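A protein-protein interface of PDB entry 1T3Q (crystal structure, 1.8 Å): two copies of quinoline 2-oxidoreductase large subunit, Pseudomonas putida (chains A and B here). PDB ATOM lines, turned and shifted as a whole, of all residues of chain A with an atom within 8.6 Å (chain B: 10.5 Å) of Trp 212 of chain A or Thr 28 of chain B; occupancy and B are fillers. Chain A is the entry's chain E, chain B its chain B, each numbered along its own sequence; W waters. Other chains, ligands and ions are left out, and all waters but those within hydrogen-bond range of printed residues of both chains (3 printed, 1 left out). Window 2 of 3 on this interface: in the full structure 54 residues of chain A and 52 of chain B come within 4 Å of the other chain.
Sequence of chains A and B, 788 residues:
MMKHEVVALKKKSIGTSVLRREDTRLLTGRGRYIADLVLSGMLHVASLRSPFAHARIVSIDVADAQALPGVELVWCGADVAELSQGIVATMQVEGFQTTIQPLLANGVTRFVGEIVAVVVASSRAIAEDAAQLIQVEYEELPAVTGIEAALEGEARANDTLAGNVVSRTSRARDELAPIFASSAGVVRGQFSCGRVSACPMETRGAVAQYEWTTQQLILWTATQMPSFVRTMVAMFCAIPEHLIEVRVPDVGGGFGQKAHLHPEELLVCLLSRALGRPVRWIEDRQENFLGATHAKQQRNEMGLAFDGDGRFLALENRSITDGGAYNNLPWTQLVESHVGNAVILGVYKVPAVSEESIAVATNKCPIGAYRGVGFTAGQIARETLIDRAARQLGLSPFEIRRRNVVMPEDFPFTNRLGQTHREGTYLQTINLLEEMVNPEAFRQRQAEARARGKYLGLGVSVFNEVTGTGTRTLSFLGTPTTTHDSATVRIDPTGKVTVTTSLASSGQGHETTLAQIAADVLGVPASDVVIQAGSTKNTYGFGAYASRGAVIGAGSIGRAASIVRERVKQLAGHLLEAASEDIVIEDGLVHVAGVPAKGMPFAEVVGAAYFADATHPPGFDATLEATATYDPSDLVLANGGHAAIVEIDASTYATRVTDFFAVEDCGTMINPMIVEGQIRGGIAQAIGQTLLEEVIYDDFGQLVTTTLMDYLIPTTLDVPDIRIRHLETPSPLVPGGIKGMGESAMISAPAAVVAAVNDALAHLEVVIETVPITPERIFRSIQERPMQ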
ATOM      1  N   GLN A 209     -33.527 -12.028  14.672  1.00  0.00           N
ATOM      2  CA  GLN A 209     -32.164 -12.373  14.304  1.00  0.00           C
ATOM      3  C   GLN A 209     -31.928 -13.852  14.584  1.00  0.00           C
ATOM      4  O   GLN A 209     -31.825 -14.272  15.737  1.00  0.00           O
ATOM      5  CB  GLN A 209     -31.166 -11.523  15.096  1.00  0.00           C
ATOM      6  CG  GLN A 209     -29.714 -11.926  14.903  1.00  0.00           C
ATOM      7  CD  GLN A 209     -28.760 -11.013  15.649  1.00  0.00           C
ATOM      8  OE1 GLN A 209     -28.256 -10.037  15.093  1.00  0.00           O
ATOM      9  NE2 GLN A 209     -28.522 -11.316  16.917  1.00  0.00           N
ATOM     10  N   TYR A 210     -31.872 -14.643  13.520  1.00  0.00           N
ATOM     11  CA  TYR A 210     -31.636 -16.072  13.657  1.00  0.00           C
ATOM     12  C   TYR A 210     -30.187 -16.365  13.287  1.00  0.00           C
ATOM     13  O   TYR A 210     -29.695 -15.902  12.254  1.00  0.00           O
ATOM     14  CB  TYR A 210     -32.567 -16.867  12.744  1.00  0.00           C
ATOM     15  CG  TYR A 210     -32.440 -18.357  12.948  1.00  0.00           C
ATOM     16  CD1 TYR A 210     -33.168 -19.009  13.941  1.00  0.00           C
ATOM     17  CD2 TYR A 210     -31.549 -19.109  12.185  1.00  0.00           C
ATOM     18  CE1 TYR A 210     -33.011 -20.375  14.171  1.00  0.00           C
ATOM     19  CE2 TYR A 210     -31.383 -20.473  12.406  1.00  0.00           C
ATOM     20  CZ  TYR A 210     -32.114 -21.098  13.397  1.00  0.00           C
ATOM     21  OH  TYR A 210     -31.948 -22.445  13.614  1.00  0.00           O
ATOM     22  N   GLU A 211     -29.511 -17.135  14.134  1.00  0.00           N
ATOM     23  CA  GLU A 211     -28.109 -17.494  13.932  1.00  0.00           C
ATOM     24  C   GLU A 211     -27.994 -18.998  13.715  1.00  0.00           C
ATOM     25  O   GLU A 211     -28.125 -19.779  14.659  1.00  0.00           O
ATOM     26  CB  GLU A 211     -27.294 -17.076  15.162  1.00  0.00           C
ATOM     27  CG  GLU A 211     -25.818 -17.435  15.089  1.00  0.00           C
ATOM     28  CD  GLU A 211     -25.185 -16.946  13.803  1.00  0.00           C
ATOM     29  OE1 GLU A 211     -24.608 -17.776  13.074  1.00  0.00           O
ATOM     30  OE2 GLU A 211     -25.273 -15.733  13.523  1.00  0.00           O
ATOM     31  N   TRP A 212     -27.732 -19.411  12.479  1.00  0.00           N
ATOM     32  CA  TRP A 212     -27.647 -20.837  12.197  1.00  0.00           C
ATOM     33  C   TRP A 212     -26.525 -21.577  12.912  1.00  0.00           C
ATOM     34  O   TRP A 212     -26.677 -22.754  13.232  1.00  0.00           O
ATOM     35  CB  TRP A 212     -27.553 -21.099  10.682  1.00  0.00           C
ATOM     36  CG  TRP A 212     -26.216 -20.819  10.057  1.00  0.00           C
ATOM     37  CD1 TRP A 212     -25.802 -19.648   9.494  1.00  0.00           C
ATOM     38  CD2 TRP A 212     -25.140 -21.748   9.889  1.00  0.00           C
ATOM     39  NE1 TRP A 212     -24.535 -19.792   8.978  1.00  0.00           N
ATOM     40  CE2 TRP A 212     -24.106 -21.072   9.208  1.00  0.00           C
ATOM     41  CE3 TRP A 212     -24.950 -23.089  10.248  1.00  0.00           C
ATOM     42  CZ2 TRP A 212     -22.896 -21.693   8.876  1.00  0.00           C
ATOM     43  CZ3 TRP A 212     -23.742 -23.708   9.915  1.00  0.00           C
ATOM     44  CH2 TRP A 212     -22.736 -23.007   9.237  1.00  0.00           C
ATOM     45  N   THR A 213     -25.406 -20.906  13.181  1.00  0.00           N
ATOM     46  CA  THR A 213     -24.292 -21.585  13.840  1.00  0.00           C
ATOM     47  C   THR A 213     -24.558 -21.979  15.296  1.00  0.00           C
ATOM     48  O   THR A 213     -23.801 -22.755  15.876  1.00  0.00           O
ATOM     49  CB  THR A 213     -22.986 -20.747  13.778  1.00  0.00           C
ATOM     50  OG1 THR A 213     -23.172 -19.494  14.448  1.00  0.00           O
ATOM     51  CG2 THR A 213     -22.587 -20.493  12.326  1.00  0.00           C
ATOM     52  N   THR A 214     -25.630 -21.446  15.880  1.00  0.00           N
ATOM     53  CA  THR A 214     -25.993 -21.761  17.262  1.00  0.00           C
ATOM     54  C   THR A 214     -27.452 -22.214  17.330  1.00  0.00           C
ATOM     55  O   THR A 214     -27.907 -22.735  18.353  1.00  0.00           O
ATOM     56  CB  THR A 214     -25.844 -20.530  18.175  1.00  0.00           C
ATOM     57  OG1 THR A 214     -26.752 -19.506  17.746  1.00  0.00           O
ATOM     58  CG2 THR A 214     -24.420 -20.005  18.125  1.00  0.00           C
ATOM     59  N   GLN A 215     -28.169 -22.012  16.227  1.00  0.00           N
ATOM     60  CA  GLN A 215     -29.581 -22.358  16.121  1.00  0.00           C
ATOM     61  C   GLN A 215     -30.417 -21.521  17.089  1.00  0.00           C
ATOM     62  O   GLN A 215     -31.548 -21.870  17.421  1.00  0.00           O
ATOM     63  CB  GLN A 215     -29.783 -23.854  16.386  1.00  0.00           C
ATOM     64  CG  GLN A 215     -29.155 -24.735  15.316  1.00  0.00           C
ATOM     65  CD  GLN A 215     -29.279 -26.212  15.628  1.00  0.00           C
ATOM     66  OE1 GLN A 215     -30.382 -26.733  15.801  1.00  0.00           O
ATOM     67  NE2 GLN A 215     -28.144 -26.899  15.703  1.00  0.00           N
ATOM     68  N   GLN A 216     -29.858 -20.396  17.526  1.00  0.00           N
ATOM     69  CA  GLN A 216     -30.559 -19.522  18.450  1.00  0.00           C
ATOM     70  C   GLN A 216     -31.232 -18.349  17.756  1.00  0.00           C
ATOM     71  O   GLN A 216     -30.722 -17.802  16.773  1.00  0.00           O
ATOM     72  CB  GLN A 216     -29.598 -19.034  19.535  1.00  0.00           C
ATOM     73  CG  GLN A 216     -29.182 -20.153  20.477  1.00  0.00           C
ATOM     74  CD  GLN A 216     -28.149 -19.725  21.497  1.00  0.00           C
ATOM     75  OE1 GLN A 216     -27.835 -20.472  22.420  1.00  0.00           O
ATOM     76  NE2 GLN A 216     -27.610 -18.522  21.335  1.00  0.00           N
ATOM     77  N   LEU A 217     -32.394 -17.983  18.283  1.00  0.00           N
ATOM     78  CA  LEU A 217     -33.196 -16.902  17.747  1.00  0.00           C
ATOM     79  C   LEU A 217     -33.436 -15.819  18.786  1.00  0.00           C
ATOM     80  O   LEU A 217     -33.807 -16.110  19.921  1.00  0.00           O
ATOM     81  CB  LEU A 217     -34.557 -17.450  17.296  1.00  0.00           C
ATOM     82  CG  LEU A 217     -35.678 -16.456  16.980  1.00  0.00           C
ATOM     83  CD1 LEU A 217     -35.331 -15.666  15.721  1.00  0.00           C
ATOM     84  CD2 LEU A 217     -36.992 -17.203  16.789  1.00  0.00           C
ATOM     85  N   SER A 272     -36.073 -14.303   9.013  1.00  0.00           N
ATOM     86  CA  SER A 272     -34.678 -14.235   9.420  1.00  0.00           C
ATOM     87  C   SER A 272     -33.994 -15.601   9.332  1.00  0.00           C
ATOM     88  O   SER A 272     -32.849 -15.702   8.887  1.00  0.00           O
ATOM     89  CB  SER A 272     -34.556 -13.687  10.845  1.00  0.00           C
ATOM     90  OG  SER A 272     -33.195 -13.650  11.249  1.00  0.00           O
ATOM     91  N   ARG A 273     -34.687 -16.655   9.749  1.00  0.00           N
ATOM     92  CA  ARG A 273     -34.097 -17.991   9.694  1.00  0.00           C
ATOM     93  C   ARG A 273     -33.842 -18.374   8.234  1.00  0.00           C
ATOM     94  O   ARG A 273     -32.788 -18.917   7.896  1.00  0.00           O
ATOM     95  CB  ARG A 273     -35.024 -19.015  10.361  1.00  0.00           C
ATOM     96  CG  ARG A 273     -34.439 -20.423  10.435  1.00  0.00           C
ATOM     97  CD  ARG A 273     -35.389 -21.395  11.130  1.00  0.00           C
ATOM     98  NE  ARG A 273     -36.677 -21.478  10.445  1.00  0.00           N
ATOM     99  CZ  ARG A 273     -37.667 -22.292  10.804  1.00  0.00           C
ATOM    100  NH1 ARG A 273     -38.803 -22.295  10.117  1.00  0.00           N
ATOM    101  NH2 ARG A 273     -37.526 -23.096  11.855  1.00  0.00           N
ATOM    102  N   ALA A 274     -34.801 -18.070   7.368  1.00  0.00           N
ATOM    103  CA  ALA A 274     -34.676 -18.376   5.941  1.00  0.00           C
ATOM    104  C   ALA A 274     -33.535 -17.617   5.264  1.00  0.00           C
ATOM    105  O   ALA A 274     -32.809 -18.176   4.438  1.00  0.00           O
ATOM    106  CB  ALA A 274     -35.992 -18.063   5.226  1.00  0.00           C
ATOM    107  N   LEU A 275     -33.369 -16.348   5.625  1.00  0.00           N
ATOM    108  CA  LEU A 275     -32.340 -15.504   5.024  1.00  0.00           C
ATOM    109  C   LEU A 275     -30.977 -15.498   5.713  1.00  0.00           C
ATOM    110  O   LEU A 275     -29.974 -15.123   5.102  1.00  0.00           O
ATOM    111  CB  LEU A 275     -32.861 -14.071   4.931  1.00  0.00           C
ATOM    112  CG  LEU A 275     -34.084 -13.903   4.030  1.00  0.00           C
ATOM    113  CD1 LEU A 275     -34.720 -12.543   4.272  1.00  0.00           C
ATOM    114  CD2 LEU A 275     -33.664 -14.068   2.566  1.00  0.00           C
ATOM    115  N   GLY A 276     -30.927 -15.909   6.974  1.00  0.00           N
ATOM    116  CA  GLY A 276     -29.656 -15.902   7.676  1.00  0.00           C
ATOM    117  C   GLY A 276     -29.203 -14.481   7.974  1.00  0.00           C
ATOM    118  O   GLY A 276     -28.011 -14.214   8.119  1.00  0.00           O
ATOM    119  N   ARG A 277     -30.161 -13.564   8.052  1.00  0.00           N
ATOM    120  CA  ARG A 277     -29.877 -12.162   8.344  1.00  0.00           C
ATOM    121  C   ARG A 277     -31.022 -11.599   9.171  1.00  0.00           C
ATOM    122  O   ARG A 277     -32.139 -12.111   9.123  1.00  0.00           O
ATOM    123  CB  ARG A 277     -29.735 -11.353   7.049  1.00  0.00           C
ATOM    124  CG  ARG A 277     -28.565 -11.792   6.176  1.00  0.00           C
ATOM    125  CD  ARG A 277     -28.476 -10.981   4.908  1.00  0.00           C
ATOM    126  NE  ARG A 277     -28.158  -9.579   5.168  1.00  0.00           N
ATOM    127  CZ  ARG A 277     -27.971  -8.670   4.217  1.00  0.00           C
ATOM    128  NH1 ARG A 277     -28.071  -9.017   2.935  1.00  0.00           N
ATOM    129  NH2 ARG A 277     -27.693  -7.416   4.542  1.00  0.00           N
ATOM    130  N   ARG B  21     -21.003 -27.936  21.024  1.00  0.00           N
ATOM    131  CA  ARG B  21     -21.958 -27.078  20.349  1.00  0.00           C
ATOM    132  C   ARG B  21     -21.350 -25.730  19.957  1.00  0.00           C
ATOM    133  O   ARG B  21     -21.823 -25.084  19.024  1.00  0.00           O
ATOM    134  CB  ARG B  21     -23.206 -26.879  21.220  1.00  0.00           C
ATOM    135  CG  ARG B  21     -22.935 -26.476  22.653  1.00  0.00           C
ATOM    136  CD  ARG B  21     -24.217 -26.521  23.485  1.00  0.00           C
ATOM    137  NE  ARG B  21     -24.804 -27.862  23.536  1.00  0.00           N
ATOM    138  CZ  ARG B  21     -25.906 -28.169  24.219  1.00  0.00           C
ATOM    139  NH1 ARG B  21     -26.374 -29.411  24.208  1.00  0.00           N
ATOM    140  NH2 ARG B  21     -26.541 -27.236  24.914  1.00  0.00           N
ATOM    141  N   GLU B  22     -20.290 -25.311  20.642  1.00  0.00           N
ATOM    142  CA  GLU B  22     -19.675 -24.030  20.308  1.00  0.00           C
ATOM    143  C   GLU B  22     -18.801 -24.070  19.055  1.00  0.00           C
ATOM    144  O   GLU B  22     -18.527 -23.031  18.451  1.00  0.00           O
ATOM    145  CB  GLU B  22     -18.851 -23.493  21.487  1.00  0.00           C
ATOM    146  CG  GLU B  22     -17.780 -24.427  22.009  1.00  0.00           C
ATOM    147  CD  GLU B  22     -18.250 -25.255  23.197  1.00  0.00           C
ATOM    148  OE1 GLU B  22     -19.227 -26.020  23.046  1.00  0.00           O
ATOM    149  OE2 GLU B  22     -17.644 -25.137  24.287  1.00  0.00           O
ATOM    150  N   ASP B  23     -18.377 -25.266  18.654  1.00  0.00           N
ATOM    151  CA  ASP B  23     -17.506 -25.420  17.491  1.00  0.00           C
ATOM    152  C   ASP B  23     -18.018 -24.825  16.192  1.00  0.00           C
ATOM    153  O   ASP B  23     -17.237 -24.282  15.416  1.00  0.00           O
ATOM    154  CB  ASP B  23     -17.195 -26.899  17.241  1.00  0.00           C
ATOM    155  CG  ASP B  23     -16.198 -27.470  18.228  1.00  0.00           C
ATOM    156  OD1 ASP B  23     -15.788 -26.753  19.170  1.00  0.00           O
ATOM    157  OD2 ASP B  23     -15.823 -28.649  18.061  1.00  0.00           O
ATOM    158  N   THR B  24     -19.322 -24.918  15.949  1.00  0.00           N
ATOM    159  CA  THR B  24     -19.867 -24.425  14.693  1.00  0.00           C
ATOM    160  C   THR B  24     -19.653 -22.935  14.463  1.00  0.00           C
ATOM    161  O   THR B  24     -19.243 -22.532  13.375  1.00  0.00           O
ATOM    162  CB  THR B  24     -21.359 -24.793  14.559  1.00  0.00           C
ATOM    163  OG1 THR B  24     -21.496 -26.215  14.695  1.00  0.00           O
ATOM    164  CG2 THR B  24     -21.893 -24.387  13.190  1.00  0.00           C
ATOM    165  N   ARG B  25     -19.900 -22.104  15.469  1.00  0.00           N
ATOM    166  CA  ARG B  25     -19.677 -20.683  15.257  1.00  0.00           C
ATOM    167  C   ARG B  25     -18.180 -20.371  15.233  1.00  0.00           C
ATOM    168  O   ARG B  25     -17.739 -19.462  14.531  1.00  0.00           O
ATOM    169  CB  ARG B  25     -20.378 -19.838  16.336  1.00  0.00           C
ATOM    170  CG  ARG B  25     -19.788 -19.908  17.736  1.00  0.00           C
ATOM    171  CD  ARG B  25     -20.492 -18.868  18.629  1.00  0.00           C
ATOM    172  NE  ARG B  25     -20.060 -18.904  20.028  1.00  0.00           N
ATOM    173  CZ  ARG B  25     -20.410 -19.845  20.902  1.00  0.00           C
ATOM    174  NH1 ARG B  25     -21.202 -20.844  20.526  1.00  0.00           N
ATOM    175  NH2 ARG B  25     -19.982 -19.775  22.159  1.00  0.00           N
ATOM    176  N   LEU B  26     -17.400 -21.140  15.985  1.00  0.00           N
ATOM    177  CA  LEU B  26     -15.959 -20.921  16.064  1.00  0.00           C
ATOM    178  C   LEU B  26     -15.186 -21.406  14.833  1.00  0.00           C
ATOM    179  O   LEU B  26     -14.017 -21.068  14.660  1.00  0.00           O
ATOM    180  CB  LEU B  26     -15.396 -21.582  17.330  1.00  0.00           C
ATOM    181  CG  LEU B  26     -15.987 -21.088  18.661  1.00  0.00           C
ATOM    182  CD1 LEU B  26     -15.391 -21.894  19.813  1.00  0.00           C
ATOM    183  CD2 LEU B  26     -15.717 -19.594  18.842  1.00  0.00           C
ATOM    184  N   LEU B  27     -15.842 -22.188  13.981  1.00  0.00           N
ATOM    185  CA  LEU B  27     -15.208 -22.707  12.765  1.00  0.00           C
ATOM    186  C   LEU B  27     -15.643 -21.921  11.532  1.00  0.00           C
ATOM    187  O   LEU B  27     -15.092 -22.100  10.442  1.00  0.00           O
ATOM    188  CB  LEU B  27     -15.573 -24.187  12.565  1.00  0.00           C
ATOM    189  CG  LEU B  27     -14.846 -25.237  13.401  1.00  0.00           C
ATOM    190  CD1 LEU B  27     -15.682 -26.511  13.487  1.00  0.00           C
ATOM    191  CD2 LEU B  27     -13.487 -25.511  12.782  1.00  0.00           C
ATOM    192  N   THR B  28     -16.631 -21.050  11.706  1.00  0.00           N
ATOM    193  CA  THR B  28     -17.152 -20.260  10.600  1.00  0.00           C
ATOM    194  C   THR B  28     -16.866 -18.770  10.717  1.00  0.00           C
ATOM    195  O   THR B  28     -17.428 -17.967   9.970  1.00  0.00           O
ATOM    196  CB  THR B  28     -18.664 -20.445  10.478  1.00  0.00           C
ATOM    197  OG1 THR B  28     -19.279 -20.140  11.739  1.00  0.00           O
ATOM    198  CG2 THR B  28     -18.992 -21.888  10.081  1.00  0.00           C
ATOM    199  N   GLY B  29     -15.993 -18.405  11.649  1.00  0.00           N
ATOM    200  CA  GLY B  29     -15.667 -17.002  11.832  1.00  0.00           C
ATOM    201  C   GLY B  29     -16.775 -16.245  12.540  1.00  0.00           C
ATOM    202  O   GLY B  29     -16.799 -15.015  12.530  1.00  0.00           O
ATOM    203  N   ARG B  30     -17.690 -16.970  13.174  1.00  0.00           N
ATOM    204  CA  ARG B  30     -18.790 -16.317  13.864  1.00  0.00           C
ATOM    205  C   ARG B  30     -18.695 -16.323  15.389  1.00  0.00           C
ATOM    206  O   ARG B  30     -19.693 -16.141  16.089  1.00  0.00           O
ATOM    207  CB  ARG B  30     -20.116 -16.914  13.410  1.00  0.00           C
ATOM    208  CG  ARG B  30     -20.365 -16.709  11.926  1.00  0.00           C
ATOM    209  CD  ARG B  30     -21.837 -16.839  11.604  1.00  0.00           C
ATOM    210  NE  ARG B  30     -22.102 -16.652  10.183  1.00  0.00           N
ATOM    211  CZ  ARG B  30     -23.317 -16.491   9.672  1.00  0.00           C
ATOM    212  NH1 ARG B  30     -23.475 -16.329   8.363  1.00  0.00           N
ATOM    213  NH2 ARG B  30     -24.373 -16.484  10.474  1.00  0.00           N
ATOM    214  N   GLY B  31     -17.492 -16.546  15.898  1.00  0.00           N
ATOM    215  CA  GLY B  31     -17.302 -16.501  17.333  1.00  0.00           C
ATOM    216  C   GLY B  31     -17.343 -15.012  17.613  1.00  0.00           C
ATOM    217  O   GLY B  31     -17.114 -14.219  16.704  1.00  0.00           O
ATOM    218  N   ARG B  32     -17.651 -14.612  18.837  1.00  0.00           N
ATOM    219  CA  ARG B  32     -17.703 -13.190  19.142  1.00  0.00           C
ATOM    220  C   ARG B  32     -16.799 -12.891  20.313  1.00  0.00           C
ATOM    221  O   ARG B  32     -17.223 -12.998  21.464  1.00  0.00           O
ATOM    222  CB  ARG B  32     -19.133 -12.760  19.470  1.00  0.00           C
ATOM    223  CG  ARG B  32     -20.081 -12.806  18.278  1.00  0.00           C
ATOM    224  N   TYR B  33     -15.557 -12.524  20.014  1.00  0.00           N
ATOM    225  CA  TYR B  33     -14.570 -12.216  21.041  1.00  0.00           C
ATOM    226  C   TYR B  33     -14.578 -10.721  21.373  1.00  0.00           C
ATOM    227  O   TYR B  33     -15.204  -9.921  20.677  1.00  0.00           O
ATOM    228  CB  TYR B  33     -13.178 -12.667  20.587  1.00  0.00           C
ATOM    229  CG  TYR B  33     -13.096 -14.140  20.223  1.00  0.00           C
ATOM    230  CD1 TYR B  33     -13.561 -14.604  18.991  1.00  0.00           C
ATOM    231  CD2 TYR B  33     -12.539 -15.068  21.109  1.00  0.00           C
ATOM    232  CE1 TYR B  33     -13.470 -15.958  18.642  1.00  0.00           C
ATOM    233  CE2 TYR B  33     -12.445 -16.424  20.774  1.00  0.00           C
ATOM    234  CZ  TYR B  33     -12.909 -16.859  19.536  1.00  0.00           C
ATOM    235  OH  TYR B  33     -12.776 -18.184  19.185  1.00  0.00           O
ATOM    236  N   ASP B  36     -13.997  -8.161  18.703  1.00  0.00           N
ATOM    237  CA  ASP B  36     -14.993  -8.172  17.632  1.00  0.00           C
ATOM    238  C   ASP B  36     -16.195  -7.292  17.946  1.00  0.00           C
ATOM    239  O   ASP B  36     -16.973  -6.956  17.055  1.00  0.00           O
ATOM    240  CB  ASP B  36     -15.482  -9.605  17.358  1.00  0.00           C
ATOM    241  CG  ASP B  36     -14.343 -10.567  17.082  1.00  0.00           C
ATOM    242  OD1 ASP B  36     -13.320 -10.111  16.536  1.00  0.00           O
ATOM    243  OD2 ASP B  36     -14.467 -11.776  17.400  1.00  0.00           O
ATOM    244  N   ASP B 250     -16.958 -14.619  23.781  1.00  0.00           N
ATOM    245  CA  ASP B 250     -16.150 -15.821  23.652  1.00  0.00           C
ATOM    246  C   ASP B 250     -14.745 -15.338  23.993  1.00  0.00           C
ATOM    247  O   ASP B 250     -14.372 -14.222  23.630  1.00  0.00           O
ATOM    248  CB  ASP B 250     -16.188 -16.359  22.217  1.00  0.00           C
ATOM    249  CG  ASP B 250     -17.532 -16.976  21.862  1.00  0.00           C
ATOM    250  OD1 ASP B 250     -18.073 -17.714  22.708  1.00  0.00           O
ATOM    251  OD2 ASP B 250     -18.039 -16.741  20.738  1.00  0.00           O
ATOM    252  N   GLU B 511     -20.028 -24.784  27.731  1.00  0.00           N
ATOM    253  CA  GLU B 511     -21.261 -24.664  26.979  1.00  0.00           C
ATOM    254  C   GLU B 511     -21.812 -26.040  26.607  1.00  0.00           C
ATOM    255  O   GLU B 511     -23.021 -26.219  26.448  1.00  0.00           O
ATOM    256  CB  GLU B 511     -20.988 -23.815  25.736  1.00  0.00           C
ATOM    257  CG  GLU B 511     -22.173 -23.538  24.856  1.00  0.00           C
ATOM    258  CD  GLU B 511     -21.867 -22.452  23.833  1.00  0.00           C
ATOM    259  OE1 GLU B 511     -22.591 -22.367  22.824  1.00  0.00           O
ATOM    260  OE2 GLU B 511     -20.902 -21.682  24.050  1.00  0.00           O
HETATM  261  O   HOH W   1     -22.479 -16.776  16.213  1.00  0.00           O
HETATM  262  O   HOH W   2     -24.509 -25.849  17.013  1.00  0.00           O
HETATM  263  O   HOH W   3     -26.281 -16.290   8.246  1.00  0.00           O
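NH2 of Arg 30 of chain B is in salt-bridge range of OE1 of Glu 211 of chain A, at 2.9 Å.
The backbone carbonyl oxygen of Thr 24 of chain B sits at hydrogen-bond distance from the side-chain hydroxyl of Thr 28 of chain B (2.9 Å). The backbone carbonyl oxygen (O) of Arg 25 of chain B is in hydrogen-bond range of the side-chain hydroxyl (OG1) of Thr 28 of chain B (3.3 Å). The backbone NH (N) of Arg 30 of chain B sits at hydrogen-bond distance from the backbone carbonyl oxygen (O) of Arg 25 of chain B (2.8 Å). NH2 of Arg 25 of chain B is in salt-bridge range of OE2 of Glu 511 of chain B (2.8 Å). OG1 of Thr 214 of chain A lies within hydrogen-bond range of O of Glu 211 of chain A (3.4 Å). The backbone NH (N) of Glu 211 of chain A is in hydrogen-bond range of the backbone carbonyl oxygen (O) of Gln 216 of chain A (3.0 Å).
Of the 16 printed residues of chain B, 4 touch a printed residue of chain A. Along chain B the printed residues that touch a printed residue of chain A span positions 24 to 30. Of the 15 printed residues of chain A, 3 touch a printed residue of chain B. Among the printed residues, Asp or Glu carboxylates within 4 Å of a Lys or Arg side-chain nitrogen of the other chain: Glu 211 of chain A with Arg 30 of chain B (2.9 Å).
Of the printed residues of chain B, Trp 212 of chain A touches Thr 24, Thr 28 and Arg 30. Of the printed residues of chain A, Thr 28 of chain B touches Trp 212 and Thr 213. Tyr 210 of chain A touches none of the printed residues of chain B. Glu 211 of chain A touches just one residue of chain B: Arg 30 (2.9 Å). No residue of chain B comes within 4 Å of Thr 214 of chain A. Gly 29 of chain B touches none of the printed residues of chain A. Printed residues of chain A within 4 Å of Thr 24 of chain B: Trp 212 and Thr 213. Printed residues of chain A within 4 Å of Arg 25 of chain B: Thr 213 (3.4 Å). Printed residues of chain A within 4 Å of Arg 30 of chain B: Glu 211, Trp 212 and Thr 213. Arg 21 of chain B touches none of the printed residues of chain A. Glu 511 of chain B touches none of the printed residues of chain A. The nearest printed residue of chain A that does not touch Thr 28 of chain B is Glu 211 of chain A (6.0 Å). The nearest printed residue of chain A that does not touch Thr 24 of chain B is Thr 214 of chain A (5.5 Å).
Water W3 bridges the backbone carbonyl oxygen (O) of Gly 276 of chain A (2.7 Å) and the guanidinium group (NH1) of Arg 30 of chain B (2.8 Å). Water W1 bridges O of Arg 30 of chain B (2.9 Å) and OG1 of Thr 213 of chain A (3.3 Å). Water W2 bridges the backbone carbonyl oxygen (O) of Thr 213 of chain A (3.4 Å) and the backbone carbonyl oxygen (O) of Arg 21 of chain B (3.4 Å).
Among the printed residues, merely in contact across the chains: Trp 212 of chain A with Thr 24 of chain B, Trp 212 of chain A with Thr 28 of chain B, Trp 212 of chain A with Arg 30 of chain B, Thr 213 of chain A with Thr 24 of chain B, Thr 213 of chain A with Arg 25 of chain B, Thr 213 of chain A with Thr 28 of chain B and Thr 213 of chain A with Arg 30 of chain B.
No position is printed for both chains.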
